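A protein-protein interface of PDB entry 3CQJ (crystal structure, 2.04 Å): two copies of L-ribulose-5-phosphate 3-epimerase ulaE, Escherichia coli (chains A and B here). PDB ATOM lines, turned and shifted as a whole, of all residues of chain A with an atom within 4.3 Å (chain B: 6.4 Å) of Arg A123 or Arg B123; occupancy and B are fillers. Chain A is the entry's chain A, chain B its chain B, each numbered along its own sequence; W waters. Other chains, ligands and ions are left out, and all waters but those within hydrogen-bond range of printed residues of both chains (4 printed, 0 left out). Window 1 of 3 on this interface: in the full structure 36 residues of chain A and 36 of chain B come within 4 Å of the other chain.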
ATOM      1  N   PRO A  83      26.471  -5.298 -17.660  1.00  0.00           N
ATOM      2  CA  PRO A  83      26.810  -3.872 -17.770  1.00  0.00           C
ATOM      3  C   PRO A  83      26.329  -3.218 -19.065  1.00  0.00           C
ATOM      4  O   PRO A  83      26.335  -1.997 -19.184  1.00  0.00           O
ATOM      5  CB  PRO A  83      28.343  -3.878 -17.722  1.00  0.00           C
ATOM      6  CG  PRO A  83      28.728  -5.185 -18.395  1.00  0.00           C
ATOM      7  CD  PRO A  83      27.623  -6.174 -17.968  1.00  0.00           C
ATOM      8  N   ALA A 117      17.536   0.241 -18.096  1.00  0.00           N
ATOM      9  CA  ALA A 117      18.931   0.397 -17.680  1.00  0.00           C
ATOM     10  C   ALA A 117      19.067   1.098 -16.318  1.00  0.00           C
ATOM     11  O   ALA A 117      19.897   0.700 -15.504  1.00  0.00           O
ATOM     12  CB  ALA A 117      19.743   1.145 -18.763  1.00  0.00           C
ATOM     13  N   GLY A 121      20.565  -1.255 -13.452  1.00  0.00           N
ATOM     14  CA  GLY A 121      21.951  -0.803 -13.344  1.00  0.00           C
ATOM     15  C   GLY A 121      22.819  -1.153 -14.539  1.00  0.00           C
ATOM     16  O   GLY A 121      24.033  -1.378 -14.395  1.00  0.00           O
ATOM     17  N   ILE A 122      22.204  -1.225 -15.721  1.00  0.00           N
ATOM     18  CA  ILE A 122      22.976  -1.392 -16.960  1.00  0.00           C
ATOM     19  C   ILE A 122      23.768  -0.096 -17.203  1.00  0.00           C
ATOM     20  O   ILE A 122      23.207   0.992 -17.127  1.00  0.00           O
ATOM     21  CB  ILE A 122      22.061  -1.758 -18.153  1.00  0.00           C
ATOM     22  CG1 ILE A 122      21.562  -3.213 -18.005  1.00  0.00           C
ATOM     23  CG2 ILE A 122      22.778  -1.524 -19.494  1.00  0.00           C
ATOM     24  CD1 ILE A 122      20.561  -3.658 -19.048  1.00  0.00           C
ATOM     25  N   ARG A 123      25.070  -0.230 -17.456  1.00  0.00           N
ATOM     26  CA  ARG A 123      25.974   0.914 -17.663  1.00  0.00           C
ATOM     27  C   ARG A 123      25.872   1.542 -19.062  1.00  0.00           C
ATOM     28  O   ARG A 123      25.930   2.765 -19.205  1.00  0.00           O
ATOM     29  CB  ARG A 123      27.443   0.502 -17.438  1.00  0.00           C
ATOM     30  CG  ARG A 123      27.724  -0.322 -16.171  1.00  0.00           C
ATOM     31  CD  ARG A 123      27.178   0.320 -14.892  1.00  0.00           C
ATOM     32  NE  ARG A 123      27.526   1.741 -14.718  1.00  0.00           N
ATOM     33  CZ  ARG A 123      27.132   2.465 -13.672  1.00  0.00           C
ATOM     34  NH1 ARG A 123      27.475   3.749 -13.558  1.00  0.00           N
ATOM     35  NH2 ARG A 123      26.408   1.896 -12.717  1.00  0.00           N
ATOM     36  N   VAL A 124      25.776   0.688 -20.078  1.00  0.00           N
ATOM     37  CA  VAL A 124      25.913   1.098 -21.461  1.00  0.00           C
ATOM     38  C   VAL A 124      24.799   0.498 -22.324  1.00  0.00           C
ATOM     39  O   VAL A 124      24.591  -0.700 -22.318  1.00  0.00           O
ATOM     40  CB  VAL A 124      27.315   0.690 -22.025  1.00  0.00           C
ATOM     41  CG1 VAL A 124      27.367   0.845 -23.558  1.00  0.00           C
ATOM     42  CG2 VAL A 124      28.437   1.527 -21.363  1.00  0.00           C
ATOM     43  N   ALA A 159      18.881  10.893 -17.686  1.00  0.00           N
ATOM     44  CA  ALA A 159      18.930   9.647 -16.922  1.00  0.00           C
ATOM     45  C   ALA A 159      20.344   9.338 -16.455  1.00  0.00           C
ATOM     46  O   ALA A 159      20.530   8.538 -15.532  1.00  0.00           O
ATOM     47  CB  ALA A 159      18.402   8.497 -17.764  1.00  0.00           C
ATOM     48  N   GLN A 160      21.321   9.978 -17.102  1.00  0.00           N
ATOM     49  CA  GLN A 160      22.755   9.693 -16.924  1.00  0.00           C
ATOM     50  C   GLN A 160      23.127   8.246 -17.259  1.00  0.00           C
ATOM     51  O   GLN A 160      23.742   7.534 -16.466  1.00  0.00           O
ATOM     52  CB  GLN A 160      23.221  10.107 -15.529  1.00  0.00           C
ATOM     53  CG  GLN A 160      23.095  11.595 -15.288  1.00  0.00           C
ATOM     54  CD  GLN A 160      23.317  11.971 -13.842  1.00  0.00           C
ATOM     55  OE1 GLN A 160      22.708  11.396 -12.946  1.00  0.00           O
ATOM     56  NE2 GLN A 160      24.194  12.945 -13.607  1.00  0.00           N
ATOM     57  N   VAL A 161      22.760   7.844 -18.470  1.00  0.00           N
ATOM     58  CA  VAL A 161      22.974   6.503 -18.985  1.00  0.00           C
ATOM     59  C   VAL A 161      23.751   6.664 -20.284  1.00  0.00           C
ATOM     60  O   VAL A 161      23.401   7.485 -21.131  1.00  0.00           O
ATOM     61  CB  VAL A 161      21.611   5.788 -19.256  1.00  0.00           C
ATOM     62  CG1 VAL A 161      21.776   4.517 -20.103  1.00  0.00           C
ATOM     63  CG2 VAL A 161      20.899   5.467 -17.932  1.00  0.00           C
ATOM     64  N   THR A 162      24.811   5.888 -20.428  1.00  0.00           N
ATOM     65  CA  THR A 162      25.661   5.960 -21.616  1.00  0.00           C
ATOM     66  C   THR A 162      25.009   5.254 -22.792  1.00  0.00           C
ATOM     67  O   THR A 162      24.558   4.096 -22.688  1.00  0.00           O
ATOM     68  CB  THR A 162      27.063   5.361 -21.340  1.00  0.00           C
ATOM     69  OG1 THR A 162      27.655   6.053 -20.238  1.00  0.00           O
ATOM     70  CG2 THR A 162      27.995   5.476 -22.569  1.00  0.00           C
ATOM     71  N   VAL B  82      18.792   7.340  -7.136  1.00  0.00           N
ATOM     72  CA  VAL B  82      20.027   7.774  -6.468  1.00  0.00           C
ATOM     73  C   VAL B  82      21.125   7.635  -7.524  1.00  0.00           C
ATOM     74  O   VAL B  82      21.909   6.675  -7.500  1.00  0.00           O
ATOM     75  CB  VAL B  82      20.336   6.978  -5.145  1.00  0.00           C
ATOM     76  CG1 VAL B  82      21.639   7.472  -4.470  1.00  0.00           C
ATOM     77  CG2 VAL B  82      19.145   7.074  -4.144  1.00  0.00           C
ATOM     78  N   PRO B  83      21.177   8.596  -8.472  1.00  0.00           N
ATOM     79  CA  PRO B  83      22.037   8.446  -9.646  1.00  0.00           C
ATOM     80  C   PRO B  83      23.467   8.924  -9.423  1.00  0.00           C
ATOM     81  O   PRO B  83      24.324   8.693 -10.263  1.00  0.00           O
ATOM     82  CB  PRO B  83      21.351   9.337 -10.682  1.00  0.00           C
ATOM     83  CG  PRO B  83      20.831  10.484  -9.852  1.00  0.00           C
ATOM     84  CD  PRO B  83      20.440   9.873  -8.496  1.00  0.00           C
ATOM     85  N   SER B  84      23.720   9.597  -8.310  1.00  0.00           N
ATOM     86  CA  SER B  84      25.050  10.112  -8.055  1.00  0.00           C
ATOM     87  C   SER B  84      25.448  10.009  -6.595  1.00  0.00           C
ATOM     88  O   SER B  84      24.593   9.994  -5.693  1.00  0.00           O
ATOM     89  CB  SER B  84      25.220  11.539  -8.590  1.00  0.00           C
ATOM     90  OG  SER B  84      24.326  12.453  -7.970  1.00  0.00           O
ATOM     91  N   MET B  85      26.758   9.933  -6.398  1.00  0.00           N
ATOM     92  CA  MET B  85      27.384   9.844  -5.103  1.00  0.00           C
ATOM     93  C   MET B  85      28.456  10.940  -4.984  1.00  0.00           C
ATOM     94  O   MET B  85      29.384  11.010  -5.794  1.00  0.00           O
ATOM     95  CB  MET B  85      28.049   8.475  -4.950  1.00  0.00           C
ATOM     96  CG  MET B  85      28.921   8.348  -3.708  1.00  0.00           C
ATOM     97  SD  MET B  85      30.118   7.000  -3.822  1.00  0.00           S
ATOM     98  CE  MET B  85      29.016   5.606  -4.092  1.00  0.00           C
ATOM     99  N   ALA B 117      28.741   1.633  -6.539  1.00  0.00           N
ATOM    100  CA  ALA B 117      27.963   2.217  -7.639  1.00  0.00           C
ATOM    101  C   ALA B 117      27.430   1.158  -8.643  1.00  0.00           C
ATOM    102  O   ALA B 117      26.281   1.255  -9.107  1.00  0.00           O
ATOM    103  CB  ALA B 117      28.762   3.323  -8.352  1.00  0.00           C
ATOM    104  N   GLN B 118      28.251   0.160  -8.960  1.00  0.00           N
ATOM    105  CA  GLN B 118      27.824  -0.994  -9.782  1.00  0.00           C
ATOM    106  C   GLN B 118      26.656  -1.753  -9.127  1.00  0.00           C
ATOM    107  O   GLN B 118      25.690  -2.108  -9.804  1.00  0.00           O
ATOM    108  CB  GLN B 118      28.963  -2.003  -9.966  1.00  0.00           C
ATOM    109  CG  GLN B 118      30.089  -1.630 -10.939  1.00  0.00           C
ATOM    110  CD  GLN B 118      31.267  -2.623 -10.878  1.00  0.00           C
ATOM    111  OE1 GLN B 118      31.966  -2.711  -9.865  1.00  0.00           O
ATOM    112  NE2 GLN B 118      31.501  -3.347 -11.974  1.00  0.00           N
ATOM    113  N   ASP B 119      26.782  -2.025  -7.826  1.00  0.00           N
ATOM    114  CA  ASP B 119      25.803  -2.828  -7.071  1.00  0.00           C
ATOM    115  C   ASP B 119      24.449  -2.134  -6.979  1.00  0.00           C
ATOM    116  O   ASP B 119      23.390  -2.765  -7.133  1.00  0.00           O
ATOM    117  CB  ASP B 119      26.319  -3.123  -5.653  1.00  0.00           C
ATOM    118  CG  ASP B 119      27.400  -4.192  -5.623  1.00  0.00           C
ATOM    119  OD1 ASP B 119      27.535  -4.946  -6.607  1.00  0.00           O
ATOM    120  OD2 ASP B 119      28.122  -4.284  -4.605  1.00  0.00           O
ATOM    121  N   VAL B 120      24.488  -0.826  -6.755  1.00  0.00           N
ATOM    122  CA  VAL B 120      23.283  -0.049  -6.448  1.00  0.00           C
ATOM    123  C   VAL B 120      22.792   0.781  -7.649  1.00  0.00           C
ATOM    124  O   VAL B 120      21.770   1.459  -7.564  1.00  0.00           O
ATOM    125  CB  VAL B 120      23.537   0.824  -5.192  1.00  0.00           C
ATOM    126  CG1 VAL B 120      22.465   1.882  -5.008  1.00  0.00           C
ATOM    127  CG2 VAL B 120      23.636  -0.073  -3.959  1.00  0.00           C
ATOM    128  N   GLY B 121      23.513   0.711  -8.768  1.00  0.00           N
ATOM    129  CA  GLY B 121      23.113   1.406  -9.999  1.00  0.00           C
ATOM    130  C   GLY B 121      23.316   2.913  -9.974  1.00  0.00           C
ATOM    131  O   GLY B 121      22.594   3.668 -10.647  1.00  0.00           O
ATOM    132  N   ILE B 122      24.281   3.361  -9.181  1.00  0.00           N
ATOM    133  CA  ILE B 122      24.693   4.759  -9.193  1.00  0.00           C
ATOM    134  C   ILE B 122      25.426   5.040 -10.520  1.00  0.00           C
ATOM    135  O   ILE B 122      26.315   4.283 -10.918  1.00  0.00           O
ATOM    136  CB  ILE B 122      25.536   5.101  -7.947  1.00  0.00           C
ATOM    137  CG1 ILE B 122      24.633   5.130  -6.694  1.00  0.00           C
ATOM    138  CG2 ILE B 122      26.263   6.445  -8.113  1.00  0.00           C
ATOM    139  CD1 ILE B 122      25.389   5.287  -5.380  1.00  0.00           C
ATOM    140  N   ARG B 123      25.016   6.116 -11.197  1.00  0.00           N
ATOM    141  CA  ARG B 123      25.514   6.477 -12.535  1.00  0.00           C
ATOM    142  C   ARG B 123      26.849   7.220 -12.515  1.00  0.00           C
ATOM    143  O   ARG B 123      27.709   6.992 -13.378  1.00  0.00           O
ATOM    144  CB  ARG B 123      24.495   7.358 -13.272  1.00  0.00           C
ATOM    145  CG  ARG B 123      23.011   6.917 -13.187  1.00  0.00           C
ATOM    146  CD  ARG B 123      22.786   5.479 -13.659  1.00  0.00           C
ATOM    147  NE  ARG B 123      23.446   5.178 -14.927  1.00  0.00           N
ATOM    148  CZ  ARG B 123      23.404   3.993 -15.531  1.00  0.00           C
ATOM    149  NH1 ARG B 123      22.710   2.984 -14.999  1.00  0.00           N
ATOM    150  NH2 ARG B 123      24.055   3.818 -16.676  1.00  0.00           N
ATOM    151  N   VAL B 124      27.000   8.118 -11.543  1.00  0.00           N
ATOM    152  CA  VAL B 124      28.115   9.069 -11.501  1.00  0.00           C
ATOM    153  C   VAL B 124      28.651   9.173 -10.068  1.00  0.00           C
ATOM    154  O   VAL B 124      27.898   9.480  -9.140  1.00  0.00           O
ATOM    155  CB  VAL B 124      27.641  10.507 -11.959  1.00  0.00           C
ATOM    156  CG1 VAL B 124      28.770  11.544 -11.825  1.00  0.00           C
ATOM    157  CG2 VAL B 124      27.102  10.497 -13.398  1.00  0.00           C
ATOM    158  N   ILE B 125      29.947   8.918  -9.895  1.00  0.00           N
ATOM    159  CA  ILE B 125      30.638   9.233  -8.650  1.00  0.00           C
ATOM    160  C   ILE B 125      31.319  10.602  -8.772  1.00  0.00           C
ATOM    161  O   ILE B 125      32.206  10.795  -9.622  1.00  0.00           O
ATOM    162  CB  ILE B 125      31.681   8.154  -8.279  1.00  0.00           C
ATOM    163  CG1 ILE B 125      30.996   6.782  -8.074  1.00  0.00           C
ATOM    164  CG2 ILE B 125      32.451   8.576  -7.031  1.00  0.00           C
ATOM    165  CD1 ILE B 125      31.981   5.613  -7.944  1.00  0.00           C
ATOM    166  N   ALA B 159      34.735  -1.082 -14.957  1.00  0.00           N
ATOM    167  CA  ALA B 159      33.395  -1.192 -14.367  1.00  0.00           C
ATOM    168  C   ALA B 159      32.351  -0.447 -15.204  1.00  0.00           C
ATOM    169  O   ALA B 159      31.137  -0.646 -15.038  1.00  0.00           O
ATOM    170  CB  ALA B 159      33.417  -0.649 -12.925  1.00  0.00           C
ATOM    171  N   GLN B 160      32.828   0.413 -16.105  1.00  0.00           N
ATOM    172  CA  GLN B 160      31.969   1.329 -16.877  1.00  0.00           C
ATOM    173  C   GLN B 160      31.120   2.228 -15.975  1.00  0.00           C
ATOM    174  O   GLN B 160      29.886   2.306 -16.096  1.00  0.00           O
ATOM    175  CB  GLN B 160      31.122   0.581 -17.907  1.00  0.00           C
ATOM    176  CG  GLN B 160      31.969  -0.113 -18.990  1.00  0.00           C
ATOM    177  CD  GLN B 160      31.147  -1.060 -19.827  1.00  0.00           C
ATOM    178  OE1 GLN B 160      30.448  -1.926 -19.297  1.00  0.00           O
ATOM    179  NE2 GLN B 160      31.223  -0.904 -21.143  1.00  0.00           N
ATOM    180  N   VAL B 161      31.810   2.906 -15.066  1.00  0.00           N
ATOM    181  CA  VAL B 161      31.195   3.798 -14.115  1.00  0.00           C
ATOM    182  C   VAL B 161      31.832   5.165 -14.334  1.00  0.00           C
ATOM    183  O   VAL B 161      33.053   5.278 -14.398  1.00  0.00           O
ATOM    184  CB  VAL B 161      31.458   3.337 -12.649  1.00  0.00           C
ATOM    185  CG1 VAL B 161      31.076   4.454 -11.629  1.00  0.00           C
ATOM    186  CG2 VAL B 161      30.689   2.041 -12.327  1.00  0.00           C
ATOM    187  N   THR B 162      30.998   6.189 -14.426  1.00  0.00           N
ATOM    188  CA  THR B 162      31.451   7.561 -14.646  1.00  0.00           C
ATOM    189  C   THR B 162      31.966   8.208 -13.374  1.00  0.00           C
ATOM    190  O   THR B 162      31.303   8.192 -12.330  1.00  0.00           O
ATOM    191  CB  THR B 162      30.309   8.457 -15.193  1.00  0.00           C
ATOM    192  OG1 THR B 162      29.760   7.857 -16.366  1.00  0.00           O
ATOM    193  CG2 THR B 162      30.832   9.849 -15.538  1.00  0.00           C
ATOM    194  N   LEU B 163      33.158   8.780 -13.489  1.00  0.00           N
ATOM    195  CA  LEU B 163      33.715   9.617 -12.452  1.00  0.00           C
ATOM    196  C   LEU B 163      33.672  11.053 -12.962  1.00  0.00           C
ATOM    197  O   LEU B 163      34.119  11.340 -14.072  1.00  0.00           O
ATOM    198  CB  LEU B 163      35.162   9.197 -12.138  1.00  0.00           C
ATOM    199  CG  LEU B 163      35.477   7.725 -11.837  1.00  0.00           C
ATOM    200  CD1 LEU B 163      36.949   7.595 -11.470  1.00  0.00           C
ATOM    201  CD2 LEU B 163      34.598   7.174 -10.702  1.00  0.00           C
ATOM    202  N   TRP B 190      35.222   7.913 -19.312  1.00  0.00           N
ATOM    203  CA  TRP B 190      34.651   7.731 -17.967  1.00  0.00           C
ATOM    204  C   TRP B 190      35.100   8.810 -16.977  1.00  0.00           C
ATOM    205  O   TRP B 190      34.705   8.808 -15.806  1.00  0.00           O
ATOM    206  CB  TRP B 190      34.913   6.301 -17.467  1.00  0.00           C
ATOM    207  CG  TRP B 190      34.279   5.247 -18.359  1.00  0.00           C
ATOM    208  CD1 TRP B 190      34.925   4.366 -19.202  1.00  0.00           C
ATOM    209  CD2 TRP B 190      32.875   4.981 -18.505  1.00  0.00           C
ATOM    210  NE1 TRP B 190      34.007   3.573 -19.847  1.00  0.00           N
ATOM    211  CE2 TRP B 190      32.741   3.928 -19.440  1.00  0.00           C
ATOM    212  CE3 TRP B 190      31.717   5.525 -17.926  1.00  0.00           C
ATOM    213  CZ2 TRP B 190      31.486   3.422 -19.827  1.00  0.00           C
ATOM    214  CZ3 TRP B 190      30.473   5.019 -18.300  1.00  0.00           C
ATOM    215  CH2 TRP B 190      30.370   3.975 -19.247  1.00  0.00           C
HETATM  216  O   HOH W   1      26.272   5.140 -17.664  1.00  0.00           O
HETATM  217  O   HOH W   2      23.342  13.513 -10.736  1.00  0.00           O
HETATM  218  O   HOH W   3      27.978   5.620 -15.718  1.00  0.00           O
HETATM  219  O   HOH W   4      25.295  -0.639 -12.165  1.00  0.00           O
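The backbone carbonyl oxygen of Ile A122 sits at hydrogen-bond distance from the guanidinium group of Arg B123 (3.0 Å). NH1 of Arg A123 sits at hydrogen-bond distance from O of Ile B122 (2.9 Å). NH1 of Arg A123 sits at hydrogen-bond distance from O of Arg B123 (3.3 Å). The backbone carbonyl oxygen of Gln B160 is in hydrogen-bond range of the guanidinium group of Arg A123, at 2.8 Å. The backbone carbonyl oxygen (O) of Gln A160 lies within hydrogen-bond range of the guanidinium group (NE) of Arg B123 (2.8 Å).
The backbone carbonyl oxygen (O) of Pro A83 is in hydrogen-bond range of the backbone NH (N) of Arg A123 (2.8 Å). The backbone carbonyl oxygen (O) of Ala A117 is in hydrogen-bond range of the backbone NH (N) of Ile A122 (3.0 Å). The backbone NH of Arg B123 sits at hydrogen-bond distance from the backbone carbonyl oxygen of Pro B83, 2.8 Å away. N of Met B85 lies within hydrogen-bond range of O of Val B124 (3.0 Å). The backbone carbonyl oxygen (O) of Ala B117 sits at hydrogen-bond distance from the backbone NH (N) of Ile B122 (2.9 Å). The backbone carbonyl oxygen of Trp B190 sits at hydrogen-bond distance from the backbone NH of Leu B163, at 2.8 Å.
Among the printed residues, pairs that only touch across the chains: Pro A83 with Gln B160 (3.3 Å), Ala A117 with Arg B123 (3.7 Å), Arg A123 with Ala B117 (3.7 Å), Arg A123 with Ala B159 (3.6 Å), Arg A123 with Val B161 (3.8 Å), Val A124 with Gln B160 (3.7 Å), Val A124 with Trp B190 (3.8 Å), Ala A159 with Arg B123 (3.8 Å), Gln A160 with Pro B83 (3.3 Å), Gln A160 with Val B124 (3.8 Å), Val A161 with Arg B123 (3.7 Å) and Thr A162 with Trp B190 (3.6 Å).
Printed residues of chain B within 4 Å of Pro A83: Gln B160. Printed residues of chain B within 4 Å of Ala A117: Arg B123 (3.7 Å). Arg A123 touches just these residues of chain B: Ala B117, Ile B122, Arg B123, Ala B159, Gln B160 and Val B161. Of chain A, only Ala A117, Ile A122, Arg A123, Ala A159, Gln A160 and Val A161 come within 4 Å of Arg B123. Of the printed residues of chain A, Val B124 touches Gln A160 (3.8 Å). Printed residues of chain A within 4 Å of Ala B159: Arg A123. Of the printed residues of chain A, Gln B160 touches Pro A83, Arg A123 and Val A124. The nearest residue of chain B that does not touch Arg A123 is Gly B121 (4.3 Å). The nearest residue of chain A that does not touch Arg B123 is Gly A121 (4.2 Å).
Of the 10 printed residues of chain A, 9 touch a printed residue of chain B. Hydrophobic or aromatic side chains of chain A within 4 Å of the printed part of chain B: Pro A83, Val A124 and Val A161. Of the 19 printed residues of chain B, 9 touch a printed residue of chain A. Hydrophobic or aromatic side chains of chain B that line the printed part of chain A: Pro B83, Val B124, Val B161 and Trp B190. Among the printed residues, 17 pairs touch across the chains. Among the printed residues, no Asp or Glu carboxylate lies within 4 Å of a Lys or Arg side-chain nitrogen of the other chain.
Ala A117 touches Arg B123, and with the chains exchanged Arg A123 touches Ala B117. Arg B123 touches its own counterpart, Arg A123. Arg A123 touches Val B161, and with the chains exchanged Val A161 touches Arg B123. Val A124 touches Gln B160, and with the chains exchanged Gln A160 touches Val B124.
Water W4 lies within hydrogen-bond range of O of Gly A121 (2.7 Å), O of Gln B118 (2.8 Å) and NH2 of Arg A123 (2.8 Å). Water W3 lies within hydrogen-bond range of the backbone carbonyl oxygen (O) of Arg B123 (2.7 Å), the guanidinium group (NH1) of Arg A123 (2.9 Å) and the side-chain hydroxyl (OG1) of Thr B162 (2.9 Å). Water W1 lies within hydrogen-bond range of the guanidinium group of Arg B123, the backbone carbonyl oxygen of Arg A123 and the side-chain hydroxyl of Thr A162. Water W2 bridges NE2 of Gln A160 (3.0 Å) and OG of Ser B84 (3.1 Å).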
